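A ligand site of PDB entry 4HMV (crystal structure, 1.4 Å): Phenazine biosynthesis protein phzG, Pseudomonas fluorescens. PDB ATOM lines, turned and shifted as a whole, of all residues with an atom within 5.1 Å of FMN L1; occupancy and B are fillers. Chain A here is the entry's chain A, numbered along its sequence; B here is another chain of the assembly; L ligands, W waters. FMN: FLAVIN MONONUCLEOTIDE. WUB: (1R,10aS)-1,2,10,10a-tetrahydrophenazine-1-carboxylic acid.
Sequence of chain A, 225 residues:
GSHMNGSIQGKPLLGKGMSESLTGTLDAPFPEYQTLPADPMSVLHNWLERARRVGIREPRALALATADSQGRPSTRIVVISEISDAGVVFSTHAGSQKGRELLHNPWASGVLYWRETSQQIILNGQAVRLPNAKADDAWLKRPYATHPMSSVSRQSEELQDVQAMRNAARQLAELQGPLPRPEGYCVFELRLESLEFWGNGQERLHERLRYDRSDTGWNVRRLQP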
ATOM      1  N   GLU A  58     -14.870   5.024 -13.965  1.00  0.00           N
ATOM      2  CA  GLU A  58     -14.358   4.438 -12.716  1.00  0.00           C
ATOM      3  C   GLU A  58     -15.412   3.602 -11.957  1.00  0.00           C
ATOM      4  O   GLU A  58     -15.751   3.865 -10.796  1.00  0.00           O
ATOM      5  CB  GLU A  58     -13.733   5.486 -11.813  1.00  0.00           C
ATOM      6  CG  GLU A  58     -12.484   6.119 -12.422  1.00  0.00           C
ATOM      7  CD  GLU A  58     -11.794   7.081 -11.474  1.00  0.00           C
ATOM      8  OE1 GLU A  58     -11.743   6.771 -10.254  1.00  0.00           O
ATOM      9  OE2 GLU A  58     -11.341   8.151 -11.947  1.00  0.00           O
ATOM     10  N   ALA A  61     -14.448   1.932  -8.324  1.00  0.00           N
ATOM     11  CA  ALA A  61     -14.064   2.766  -7.200  1.00  0.00           C
ATOM     12  C   ALA A  61     -15.041   2.498  -6.061  1.00  0.00           C
ATOM     13  O   ALA A  61     -16.166   2.969  -6.055  1.00  0.00           O
ATOM     14  CB  ALA A  61     -14.100   4.240  -7.612  1.00  0.00           C
ATOM     15  N   THR A  75     -14.060   5.328   6.415  1.00  0.00           N
ATOM     16  CA  THR A  75     -14.278   5.110   5.002  1.00  0.00           C
ATOM     17  C   THR A  75     -13.163   5.688   4.143  1.00  0.00           C
ATOM     18  O   THR A  75     -12.432   6.582   4.566  1.00  0.00           O
ATOM     19  CB  THR A  75     -15.608   5.712   4.499  1.00  0.00           C
ATOM     20  OG1 THR A  75     -15.633   7.132   4.757  1.00  0.00           O
ATOM     21  CG2 THR A  75     -16.824   5.069   5.147  1.00  0.00           C
ATOM     22  N   ARG A  76     -13.060   5.166   2.929  1.00  0.00           N
ATOM     23  CA  ARG A  76     -12.143   5.673   1.900  1.00  0.00           C
ATOM     24  C   ARG A  76     -12.449   4.934   0.608  1.00  0.00           C
ATOM     25  O   ARG A  76     -13.069   3.873   0.637  1.00  0.00           O
ATOM     26  CB  ARG A  76     -10.671   5.446   2.281  1.00  0.00           C
ATOM     27  CG  ARG A  76     -10.198   3.986   2.129  1.00  0.00           C
ATOM     28  CD  ARG A  76     -10.812   3.044   3.144  1.00  0.00           C
ATOM     29  NE  ARG A  76     -10.430   3.381   4.507  1.00  0.00           N
ATOM     30  CZ  ARG A  76     -10.963   2.874   5.598  1.00  0.00           C
ATOM     31  NH1 ARG A  76     -10.432   3.191   6.761  1.00  0.00           N
ATOM     32  NH2 ARG A  76     -12.005   2.066   5.553  1.00  0.00           N
ATOM     33  N   ILE A  77     -11.970   5.460  -0.526  1.00  0.00           N
ATOM     34  CA  ILE A  77     -12.075   4.741  -1.783  1.00  0.00           C
ATOM     35  C   ILE A  77     -10.913   3.750  -1.927  1.00  0.00           C
ATOM     36  O   ILE A  77      -9.755   4.073  -1.676  1.00  0.00           O
ATOM     37  CB  ILE A  77     -12.043   5.703  -2.989  1.00  0.00           C
ATOM     38  CG1 ILE A  77     -13.209   6.700  -2.916  1.00  0.00           C
ATOM     39  CG2 ILE A  77     -12.110   4.929  -4.308  1.00  0.00           C
ATOM     40  CD1 ILE A  77     -14.630   6.116  -2.990  1.00  0.00           C
ATOM     41  N   VAL A  78     -11.235   2.528  -2.370  1.00  0.00           N
ATOM     42  CA  VAL A  78     -10.247   1.575  -2.882  1.00  0.00           C
ATOM     43  C   VAL A  78     -10.752   1.052  -4.217  1.00  0.00           C
ATOM     44  O   VAL A  78     -11.946   1.138  -4.532  1.00  0.00           O
ATOM     45  CB  VAL A  78      -9.955   0.395  -1.901  1.00  0.00           C
ATOM     46  CG1 VAL A  78      -9.409   0.920  -0.569  1.00  0.00           C
ATOM     47  CG2 VAL A  78     -11.201  -0.518  -1.720  1.00  0.00           C
ATOM     48  N   VAL A  79      -9.852   0.502  -5.027  1.00  0.00           N
ATOM     49  CA  VAL A  79     -10.232  -0.078  -6.291  1.00  0.00           C
ATOM     50  C   VAL A  79     -10.363  -1.591  -6.182  1.00  0.00           C
ATOM     51  O   VAL A  79      -9.480  -2.269  -5.641  1.00  0.00           O
ATOM     52  CB  VAL A  79      -9.172   0.218  -7.369  1.00  0.00           C
ATOM     53  CG1 VAL A  79      -9.466  -0.557  -8.643  1.00  0.00           C
ATOM     54  CG2 VAL A  79      -9.078   1.706  -7.623  1.00  0.00           C
ATOM     55  N   SER A  91      -6.205  -4.316  -2.929  1.00  0.00           N
ATOM     56  CA  SER A  91      -4.905  -4.256  -2.277  1.00  0.00           C
ATOM     57  C   SER A  91      -4.781  -3.002  -1.442  1.00  0.00           C
ATOM     58  O   SER A  91      -5.436  -1.998  -1.705  1.00  0.00           O
ATOM     59  CB  SER A  91      -3.783  -4.288  -3.313  1.00  0.00           C
ATOM     60  OG  SER A  91      -3.789  -5.515  -4.008  1.00  0.00           O
ATOM     61  N   THR A  92      -3.918  -3.054  -0.446  1.00  0.00           N
ATOM     62  CA  THR A  92      -3.689  -1.903   0.418  1.00  0.00           C
ATOM     63  C   THR A  92      -2.422  -2.119   1.236  1.00  0.00           C
ATOM     64  O   THR A  92      -1.669  -3.060   0.979  1.00  0.00           O
ATOM     65  CB  THR A  92      -4.916  -1.628   1.326  1.00  0.00           C
ATOM     66  OG1 THR A  92      -4.798  -0.326   1.894  1.00  0.00           O
ATOM     67  CG2 THR A  92      -5.062  -2.674   2.412  1.00  0.00           C
ATOM     68  N   HIS A  93      -2.150  -1.228   2.184  1.00  0.00           N
ATOM     69  CA  HIS A  93      -1.074  -1.449   3.162  1.00  0.00           C
ATOM     70  C   HIS A  93      -1.633  -1.898   4.508  1.00  0.00           C
ATOM     71  O   HIS A  93      -2.600  -1.330   5.026  1.00  0.00           O
ATOM     72  CB  HIS A  93      -0.239  -0.191   3.300  1.00  0.00           C
ATOM     73  CG  HIS A  93       0.467   0.171   2.030  1.00  0.00           C
ATOM     74  ND1 HIS A  93       1.774  -0.189   1.771  1.00  0.00           N
ATOM     75  CD2 HIS A  93       0.032   0.818   0.926  1.00  0.00           C
ATOM     76  CE1 HIS A  93       2.122   0.237   0.572  1.00  0.00           C
ATOM     77  NE2 HIS A  93       1.081   0.847   0.030  1.00  0.00           N
ATOM     78  N   SER A  96      -2.068   0.661   7.345  1.00  0.00           N
ATOM     79  CA  SER A  96      -3.023   1.762   7.145  1.00  0.00           C
ATOM     80  C   SER A  96      -4.122   1.678   8.176  1.00  0.00           C
ATOM     81  O   SER A  96      -4.232   0.681   8.891  1.00  0.00           O
ATOM     82  CB  SER A  96      -3.606   1.703   5.729  1.00  0.00           C
ATOM     83  OG  SER A  96      -4.405   0.557   5.561  1.00  0.00           O
ATOM     84  N   GLN A  97      -4.990   2.701   8.221  1.00  0.00           N
ATOM     85  CA  GLN A  97      -6.136   2.630   9.134  1.00  0.00           C
ATOM     86  C   GLN A  97      -7.044   1.443   8.800  1.00  0.00           C
ATOM     87  O   GLN A  97      -7.492   0.729   9.693  1.00  0.00           O
ATOM     88  CB  GLN A  97      -6.934   3.931   9.137  1.00  0.00           C
ATOM     89  CG  GLN A  97      -8.119   3.864  10.083  1.00  0.00           C
ATOM     90  CD  GLN A  97      -8.752   5.207  10.352  1.00  0.00           C
ATOM     91  OE1 GLN A  97      -8.319   6.250   9.873  1.00  0.00           O
ATOM     92  NE2 GLN A  97      -9.777   5.193  11.148  1.00  0.00           N
ATOM     93  N   LYS A  98      -7.325   1.237   7.520  1.00  0.00           N
ATOM     94  CA  LYS A  98      -8.228   0.156   7.149  1.00  0.00           C
ATOM     95  C   LYS A  98      -7.579  -1.194   7.489  1.00  0.00           C
ATOM     96  O   LYS A  98      -8.261  -2.136   7.867  1.00  0.00           O
ATOM     97  CB  LYS A  98      -8.630   0.248   5.654  1.00  0.00           C
ATOM     98  CG  LYS A  98      -7.679  -0.415   4.652  1.00  0.00           C
ATOM     99  CD  LYS A  98      -7.955  -0.018   3.222  1.00  0.00           C
ATOM    100  CE  LYS A  98      -7.556   1.427   2.876  1.00  0.00           C
ATOM    101  NZ  LYS A  98      -6.156   1.778   3.319  1.00  0.00           N
ATOM    102  N   GLY A  99      -6.274  -1.277   7.318  1.00  0.00           N
ATOM    103  CA  GLY A  99      -5.572  -2.517   7.582  1.00  0.00           C
ATOM    104  C   GLY A  99      -5.605  -2.851   9.059  1.00  0.00           C
ATOM    105  O   GLY A  99      -5.799  -4.019   9.449  1.00  0.00           O
ATOM    106  N   GLN A 155       1.694   4.111   4.660  1.00  0.00           N
ATOM    107  CA  GLN A 155       0.373   4.640   4.437  1.00  0.00           C
ATOM    108  C   GLN A 155      -0.371   4.976   5.736  1.00  0.00           C
ATOM    109  O   GLN A 155      -0.516   4.146   6.612  1.00  0.00           O
ATOM    110  CB  GLN A 155      -0.423   3.664   3.559  1.00  0.00           C
ATOM    111  CG  GLN A 155      -1.769   4.173   3.074  1.00  0.00           C
ATOM    112  CD  GLN A 155      -2.475   3.163   2.188  1.00  0.00           C
ATOM    113  OE1 GLN A 155      -2.858   2.104   2.652  1.00  0.00           O
ATOM    114  NE2 GLN A 155      -2.609   3.486   0.918  1.00  0.00           N
ATOM    115  N   SER A 156      -0.863   6.222   5.813  1.00  0.00           N
ATOM    116  CA  SER A 156      -1.715   6.739   6.891  1.00  0.00           C
ATOM    117  C   SER A 156      -0.988   7.125   8.178  1.00  0.00           C
ATOM    118  O   SER A 156      -1.621   7.678   9.089  1.00  0.00           O
ATOM    119  CB  SER A 156      -2.916   5.827   7.172  1.00  0.00           C
ATOM    120  OG  SER A 156      -3.517   5.435   5.963  1.00  0.00           O
ATOM    121  N   SER B  21      -6.228   3.478 -12.119  1.00  0.00           N
ATOM    122  CA  SER B  21      -7.643   3.666 -12.390  1.00  0.00           C
ATOM    123  C   SER B  21      -8.086   5.130 -12.400  1.00  0.00           C
ATOM    124  O   SER B  21      -9.184   5.386 -12.894  1.00  0.00           O
ATOM    125  CB  SER B  21      -8.524   2.885 -11.406  1.00  0.00           C
ATOM    126  OG  SER B  21      -8.620   3.547 -10.167  1.00  0.00           O
ATOM    127  N   LEU B  22      -7.260   6.066 -11.890  1.00  0.00           N
ATOM    128  CA  LEU B  22      -7.676   7.475 -11.815  1.00  0.00           C
ATOM    129  C   LEU B  22      -7.795   8.113 -13.179  1.00  0.00           C
ATOM    130  O   LEU B  22      -6.920   8.005 -14.014  1.00  0.00           O
ATOM    131  CB  LEU B  22      -6.750   8.369 -10.977  1.00  0.00           C
ATOM    132  CG  LEU B  22      -6.446   8.153  -9.511  1.00  0.00           C
ATOM    133  CD1 LEU B  22      -5.285   9.063  -9.104  1.00  0.00           C
ATOM    134  CD2 LEU B  22      -7.596   8.442  -8.648  1.00  0.00           C
ATOM    135  N   TYR B 113     -16.262  11.405  -3.309  1.00  0.00           N
ATOM    136  CA  TYR B 113     -15.189  11.164  -4.263  1.00  0.00           C
ATOM    137  C   TYR B 113     -15.596  11.799  -5.579  1.00  0.00           C
ATOM    138  O   TYR B 113     -16.652  11.477  -6.132  1.00  0.00           O
ATOM    139  CB  TYR B 113     -14.897   9.652  -4.448  1.00  0.00           C
ATOM    140  CG  TYR B 113     -13.915   9.392  -5.593  1.00  0.00           C
ATOM    141  CD1 TYR B 113     -12.750  10.122  -5.704  1.00  0.00           C
ATOM    142  CD2 TYR B 113     -14.167   8.428  -6.571  1.00  0.00           C
ATOM    143  CE1 TYR B 113     -11.866   9.942  -6.775  1.00  0.00           C
ATOM    144  CE2 TYR B 113     -13.281   8.214  -7.622  1.00  0.00           C
ATOM    145  CZ  TYR B 113     -12.145   8.974  -7.715  1.00  0.00           C
ATOM    146  OH  TYR B 113     -11.280   8.781  -8.766  1.00  0.00           O
ATOM    147  N   GLN B 120     -10.963  13.366  -2.760  1.00  0.00           N
ATOM    148  CA  GLN B 120     -11.839  12.700  -1.794  1.00  0.00           C
ATOM    149  C   GLN B 120     -11.951  13.550  -0.567  1.00  0.00           C
ATOM    150  O   GLN B 120     -11.005  14.234  -0.174  1.00  0.00           O
ATOM    151  CB  GLN B 120     -11.287  11.350  -1.234  1.00  0.00           C
ATOM    152  CG  GLN B 120     -10.887  10.295  -2.098  1.00  0.00           C
ATOM    153  CD  GLN B 120     -10.480   9.097  -1.204  1.00  0.00           C
ATOM    154  OE1 GLN B 120     -11.311   8.293  -0.724  1.00  0.00           O
ATOM    155  NE2 GLN B 120      -9.220   8.997  -0.964  1.00  0.00           N
ATOM    156  N   GLU B 196     -10.737  14.218   6.531  1.00  0.00           N
ATOM    157  CA  GLU B 196      -9.564  14.190   5.684  1.00  0.00           C
ATOM    158  C   GLU B 196      -9.912  14.763   4.310  1.00  0.00           C
ATOM    159  O   GLU B 196     -10.938  14.391   3.725  1.00  0.00           O
ATOM    160  CB  GLU B 196      -8.972  12.770   5.528  1.00  0.00           C
ATOM    161  CG  GLU B 196      -7.763  12.744   4.598  1.00  0.00           C
ATOM    162  CD  GLU B 196      -7.190  11.367   4.315  1.00  0.00           C
ATOM    163  OE1 GLU B 196      -7.252  10.486   5.215  1.00  0.00           O
ATOM    164  OE2 GLU B 196      -6.651  11.206   3.192  1.00  0.00           O
ATOM    165  N   TRP B 198      -8.289  14.731   0.576  1.00  0.00           N
ATOM    166  CA  TRP B 198      -7.341  13.946  -0.210  1.00  0.00           C
ATOM    167  C   TRP B 198      -7.300  14.479  -1.637  1.00  0.00           C
ATOM    168  O   TRP B 198      -8.345  14.605  -2.290  1.00  0.00           O
ATOM    169  CB  TRP B 198      -7.812  12.503  -0.227  1.00  0.00           C
ATOM    170  CG  TRP B 198      -6.879  11.482  -0.859  1.00  0.00           C
ATOM    171  CD1 TRP B 198      -6.122  10.559  -0.189  1.00  0.00           C
ATOM    172  CD2 TRP B 198      -6.655  11.232  -2.274  1.00  0.00           C
ATOM    173  NE1 TRP B 198      -5.441   9.752  -1.088  1.00  0.00           N
ATOM    174  CE2 TRP B 198      -5.768  10.136  -2.372  1.00  0.00           C
ATOM    175  CE3 TRP B 198      -7.133  11.808  -3.462  1.00  0.00           C
ATOM    176  CZ2 TRP B 198      -5.326   9.637  -3.601  1.00  0.00           C
ATOM    177  CZ3 TRP B 198      -6.680  11.300  -4.688  1.00  0.00           C
ATOM    178  CH2 TRP B 198      -5.800  10.210  -4.731  1.00  0.00           C
ATOM    179  N   ARG B 208      -2.743  14.423   1.669  1.00  0.00           N
ATOM    180  CA  ARG B 208      -3.726  14.028   2.661  1.00  0.00           C
ATOM    181  C   ARG B 208      -3.632  14.976   3.837  1.00  0.00           C
ATOM    182  O   ARG B 208      -2.647  14.995   4.572  1.00  0.00           O
ATOM    183  CB  ARG B 208      -3.418  12.623   3.126  1.00  0.00           C
ATOM    184  CG  ARG B 208      -3.404  11.569   2.015  1.00  0.00           C
ATOM    185  CD  ARG B 208      -3.162  10.172   2.546  1.00  0.00           C
ATOM    186  NE  ARG B 208      -4.262   9.769   3.411  1.00  0.00           N
ATOM    187  CZ  ARG B 208      -4.299   8.626   4.100  1.00  0.00           C
ATOM    188  NH1 ARG B 208      -3.296   7.773   4.058  1.00  0.00           N
ATOM    189  NH2 ARG B 208      -5.370   8.340   4.842  1.00  0.00           N
ATOM    190  N   PRO B 225       0.860   8.909   2.004  1.00  0.00           N
ATOM    191  CA  PRO B 225      -0.087   8.394   1.004  1.00  0.00           C
ATOM    192  C   PRO B 225      -0.229   6.900   0.943  1.00  0.00           C
ATOM    193  O   PRO B 225      -1.294   6.416   0.491  1.00  0.00           O
ATOM    194  CB  PRO B 225       0.471   8.942  -0.306  1.00  0.00           C
ATOM    195  CG  PRO B 225       1.914   9.167  -0.036  1.00  0.00           C
ATOM    196  CD  PRO B 225       1.995   9.604   1.377  1.00  0.00           C
ATOM    197  OXT PRO B 225       0.707   6.178   1.334  1.00  0.00           O
HETATM  198  N1  FMN L   1      -5.656   3.011  -1.338  1.00  0.00           N
HETATM  199  C2  FMN L   1      -5.322   1.691  -1.241  1.00  0.00           C
HETATM  200  O2  FMN L   1      -4.682   1.286  -0.280  1.00  0.00           O
HETATM  201  N3  FMN L   1      -5.774   0.798  -2.192  1.00  0.00           N
HETATM  202  C4  FMN L   1      -6.511   1.195  -3.282  1.00  0.00           C
HETATM  203  O4  FMN L   1      -6.926   0.363  -4.085  1.00  0.00           O
HETATM  204  C4A FMN L   1      -6.797   2.552  -3.400  1.00  0.00           C
HETATM  205  N5  FMN L   1      -7.525   3.008  -4.466  1.00  0.00           N
HETATM  206  C5A FMN L   1      -7.859   4.356  -4.554  1.00  0.00           C
HETATM  207  C6  FMN L   1      -8.646   4.810  -5.616  1.00  0.00           C
HETATM  208  C7  FMN L   1      -9.029   6.143  -5.684  1.00  0.00           C
HETATM  209  C7M FMN L   1      -9.861   6.548  -6.853  1.00  0.00           C
HETATM  210  C8  FMN L   1      -8.595   7.036  -4.709  1.00  0.00           C
HETATM  211  C8M FMN L   1      -8.990   8.482  -4.758  1.00  0.00           C
HETATM  212  C9  FMN L   1      -7.846   6.581  -3.623  1.00  0.00           C
HETATM  213  C9A FMN L   1      -7.454   5.235  -3.560  1.00  0.00           C
HETATM  214  N10 FMN L   1      -6.676   4.753  -2.505  1.00  0.00           N
HETATM  215  C10 FMN L   1      -6.392   3.417  -2.410  1.00  0.00           C
HETATM  216  C1' FMN L   1      -6.263   5.637  -1.377  1.00  0.00           C
HETATM  217  C2' FMN L   1      -7.304   5.466  -0.242  1.00  0.00           C
HETATM  218  O2' FMN L   1      -8.495   6.196  -0.548  1.00  0.00           O
HETATM  219  C3' FMN L   1      -6.794   5.914   1.122  1.00  0.00           C
HETATM  220  O3' FMN L   1      -6.265   7.249   1.060  1.00  0.00           O
HETATM  221  C4' FMN L   1      -5.684   5.016   1.672  1.00  0.00           C
HETATM  222  O4' FMN L   1      -5.919   3.659   1.288  1.00  0.00           O
HETATM  223  C5' FMN L   1      -5.579   5.189   3.183  1.00  0.00           C
HETATM  224  O5' FMN L   1      -6.818   4.865   3.771  1.00  0.00           O
HETATM  225  P   FMN L   1      -6.968   4.639   5.353  1.00  0.00           P
HETATM  226  O1P FMN L   1      -6.511   3.236   5.639  1.00  0.00           O
HETATM  227  O2P FMN L   1      -6.075   5.660   6.031  1.00  0.00           O
HETATM  228  O3P FMN L   1      -8.431   4.911   5.656  1.00  0.00           O
HETATM  229  O01 WUB L   2      -6.237   3.199  -9.359  1.00  0.00           O
HETATM  230  C02 WUB L   2      -5.171   3.152  -8.648  1.00  0.00           C
HETATM  231  O03 WUB L   2      -3.955   2.759  -8.770  1.00  0.00           O
HETATM  232  C04 WUB L   2      -5.389   3.766  -7.297  1.00  0.00           C
HETATM  233  C05 WUB L   2      -5.430   5.282  -7.423  1.00  0.00           C
HETATM  234  C06 WUB L   2      -5.033   6.150  -6.239  1.00  0.00           C
HETATM  235  C07 WUB L   2      -4.383   5.625  -5.166  1.00  0.00           C
HETATM  236  C08 WUB L   2      -4.081   4.175  -5.157  1.00  0.00           C
HETATM  237  N09 WUB L   2      -3.520   3.661  -4.053  1.00  0.00           N
HETATM  238  C10 WUB L   2      -3.225   2.290  -3.961  1.00  0.00           C
HETATM  239  C11 WUB L   2      -2.514   1.831  -2.836  1.00  0.00           C
HETATM  240  C12 WUB L   2      -2.257   0.461  -2.697  1.00  0.00           C
HETATM  241  C13 WUB L   2      -2.691  -0.418  -3.667  1.00  0.00           C
HETATM  242  C14 WUB L   2      -3.399   0.038  -4.756  1.00  0.00           C
HETATM  243  C15 WUB L   2      -3.668   1.434  -4.909  1.00  0.00           C
HETATM  244  N16 WUB L   2      -4.400   1.896  -6.046  1.00  0.00           N
HETATM  245  C17 WUB L   2      -4.280   3.302  -6.392  1.00  0.00           C
HETATM  246  O   HOH W   1     -10.645   6.717   6.528  1.00  0.00           O
HETATM  247  O   HOH W   2      -6.593   7.366   8.073  1.00  0.00           O
HETATM  248  O   HOH W   3      -6.909  -2.277  -4.880  1.00  0.00           O
HETATM  249  O   HOH W   4      -9.012   7.482   4.869  1.00  0.00           O
HETATM  250  O   HOH W   5      -7.934   8.793   2.373  1.00  0.00           O
HETATM  251  O   HOH W   6      -3.643   7.772  -0.109  1.00  0.00           O
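The side-chain hydroxyl (OG) of Ser 156 lies within hydrogen-bond range of an oxygen (O2P) of FMN L1, at 2.6 Å. An oxygen (O2) of FMN L1 sits at hydrogen-bond distance from the side-chain hydroxyl of Thr 92. The backbone carbonyl oxygen (O) of Ile 77 lies within hydrogen-bond range of an oxygen (O2') of FMN L1 (2.7 Å). The backbone NH (N) of Lys 98 lies within hydrogen-bond range of an oxygen (O1P) of FMN L1, 2.9 Å away. The side-chain amino group (NZ) of Lys 98 is in salt-bridge range of an oxygen (O1P) of FMN L1 (2.8 Å). O3P of FMN L1 is in salt-bridge range of NE of Arg 76, 2.8 Å away. O of Ser 91 sits at hydrogen-bond distance from N3 of FMN L1. The side-chain amide nitrogen (NE2) of Gln 120 of chain B sits at hydrogen-bond distance from an oxygen (O2') of FMN L1, at 2.9 Å. An oxygen (O2P) of FMN L1 is in salt-bridge range of the guanidinium group (NH2) of Arg 208 of chain B, 3.0 Å away. O1P of FMN L1 sits at hydrogen-bond distance from N of Gln 97, 3.0 Å away. An oxygen (O4) of FMN L1 lies within hydrogen-bond range of the backbone NH (N) of Val 79. The side-chain amide nitrogen (NE2) of Gln 155 is in hydrogen-bond range of an oxygen (O2) of FMN L1, at 3.3 Å. OG of Ser 96 sits close to O1P of FMN L1 (3.4 Å). The indole nitrogen (NE1) of Trp 198 of chain B is in hydrogen-bond range of an oxygen (O3') of FMN L1, 3.4 Å away. An oxygen (O01) of WUB L2 is in hydrogen-bond range of the backbone NH (N) of Ser 21 of chain B, at 2.8 Å. O01 of WUB L2 is in hydrogen-bond range of OG of Ser 21 of chain B (2.5 Å).
The guanidinium group (NH1) of Arg 208 of chain B lies within hydrogen-bond range of the side-chain hydroxyl (OG) of Ser 156, at 3.0 Å. NZ of Lys 98 sits at hydrogen-bond distance from OG1 of Thr 92, 2.9 Å away. The side-chain hydroxyl of Thr 92 lies within hydrogen-bond range of the side-chain amide oxygen of Gln 155 (3.2 Å). The side-chain amide oxygen (OE1) of Gln 120 of chain B lies within hydrogen-bond range of the backbone NH (N) of Ile 77, at 2.9 Å. NZ of Lys 98 sits at hydrogen-bond distance from OE1 of Gln 155 (3.4 Å). The guanidinium group (NE) of Arg 208 of chain B is in salt-bridge range of the side-chain carboxylate (OE2) of Glu 196 of chain B, at 2.8 Å. The side-chain hydroxyl (OH) of Tyr 113 of chain B sits at hydrogen-bond distance from the side-chain carboxylate (OE1) of Glu 58. The side-chain hydroxyl (OG) of Ser 96 lies within hydrogen-bond range of the backbone NH (N) of Gly 99, at 3.2 Å.
Residues that only touch FMN L1: Tyr 113 of chain B (3.3 Å), Leu 22 of chain B (3.5 Å), Val 78 (3.5 Å) and Glu 58 (3.9 Å). Of the 24 residues printed, 17 come within 4 Å of FMN L1. The nearest printed residue that does not touch FMN L1 is His 93 (4.3 Å).
Water W5 bridges an oxygen (O3') of FMN L1 (2.6 Å) and the side-chain carboxylate of Glu 196 of chain B (2.9 Å). Water W2 bridges O2P of FMN L1 (2.7 Å) and OE1 of Gln 97 (2.7 Å). Water W4 lies within hydrogen-bond range of O3P of FMN L1 and OE1 of Glu 196 of chain B. Water W3 lies within hydrogen-bond range of the backbone carbonyl oxygen (O) of Val 79 (2.7 Å), an oxygen (O4) of FMN L1 (2.8 Å) and the backbone NH (N) of Ser 91 (2.9 Å). Water W6 lies within hydrogen-bond range of O of Pro 225 of chain B (2.8 Å), NE1 of Trp 198 of chain B (2.8 Å) and O3' of FMN L1 (2.9 Å). Water W1 bridges the backbone carbonyl oxygen of Thr 75 (2.7 Å) and an oxygen (O3P) of FMN L1 (3.0 Å).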
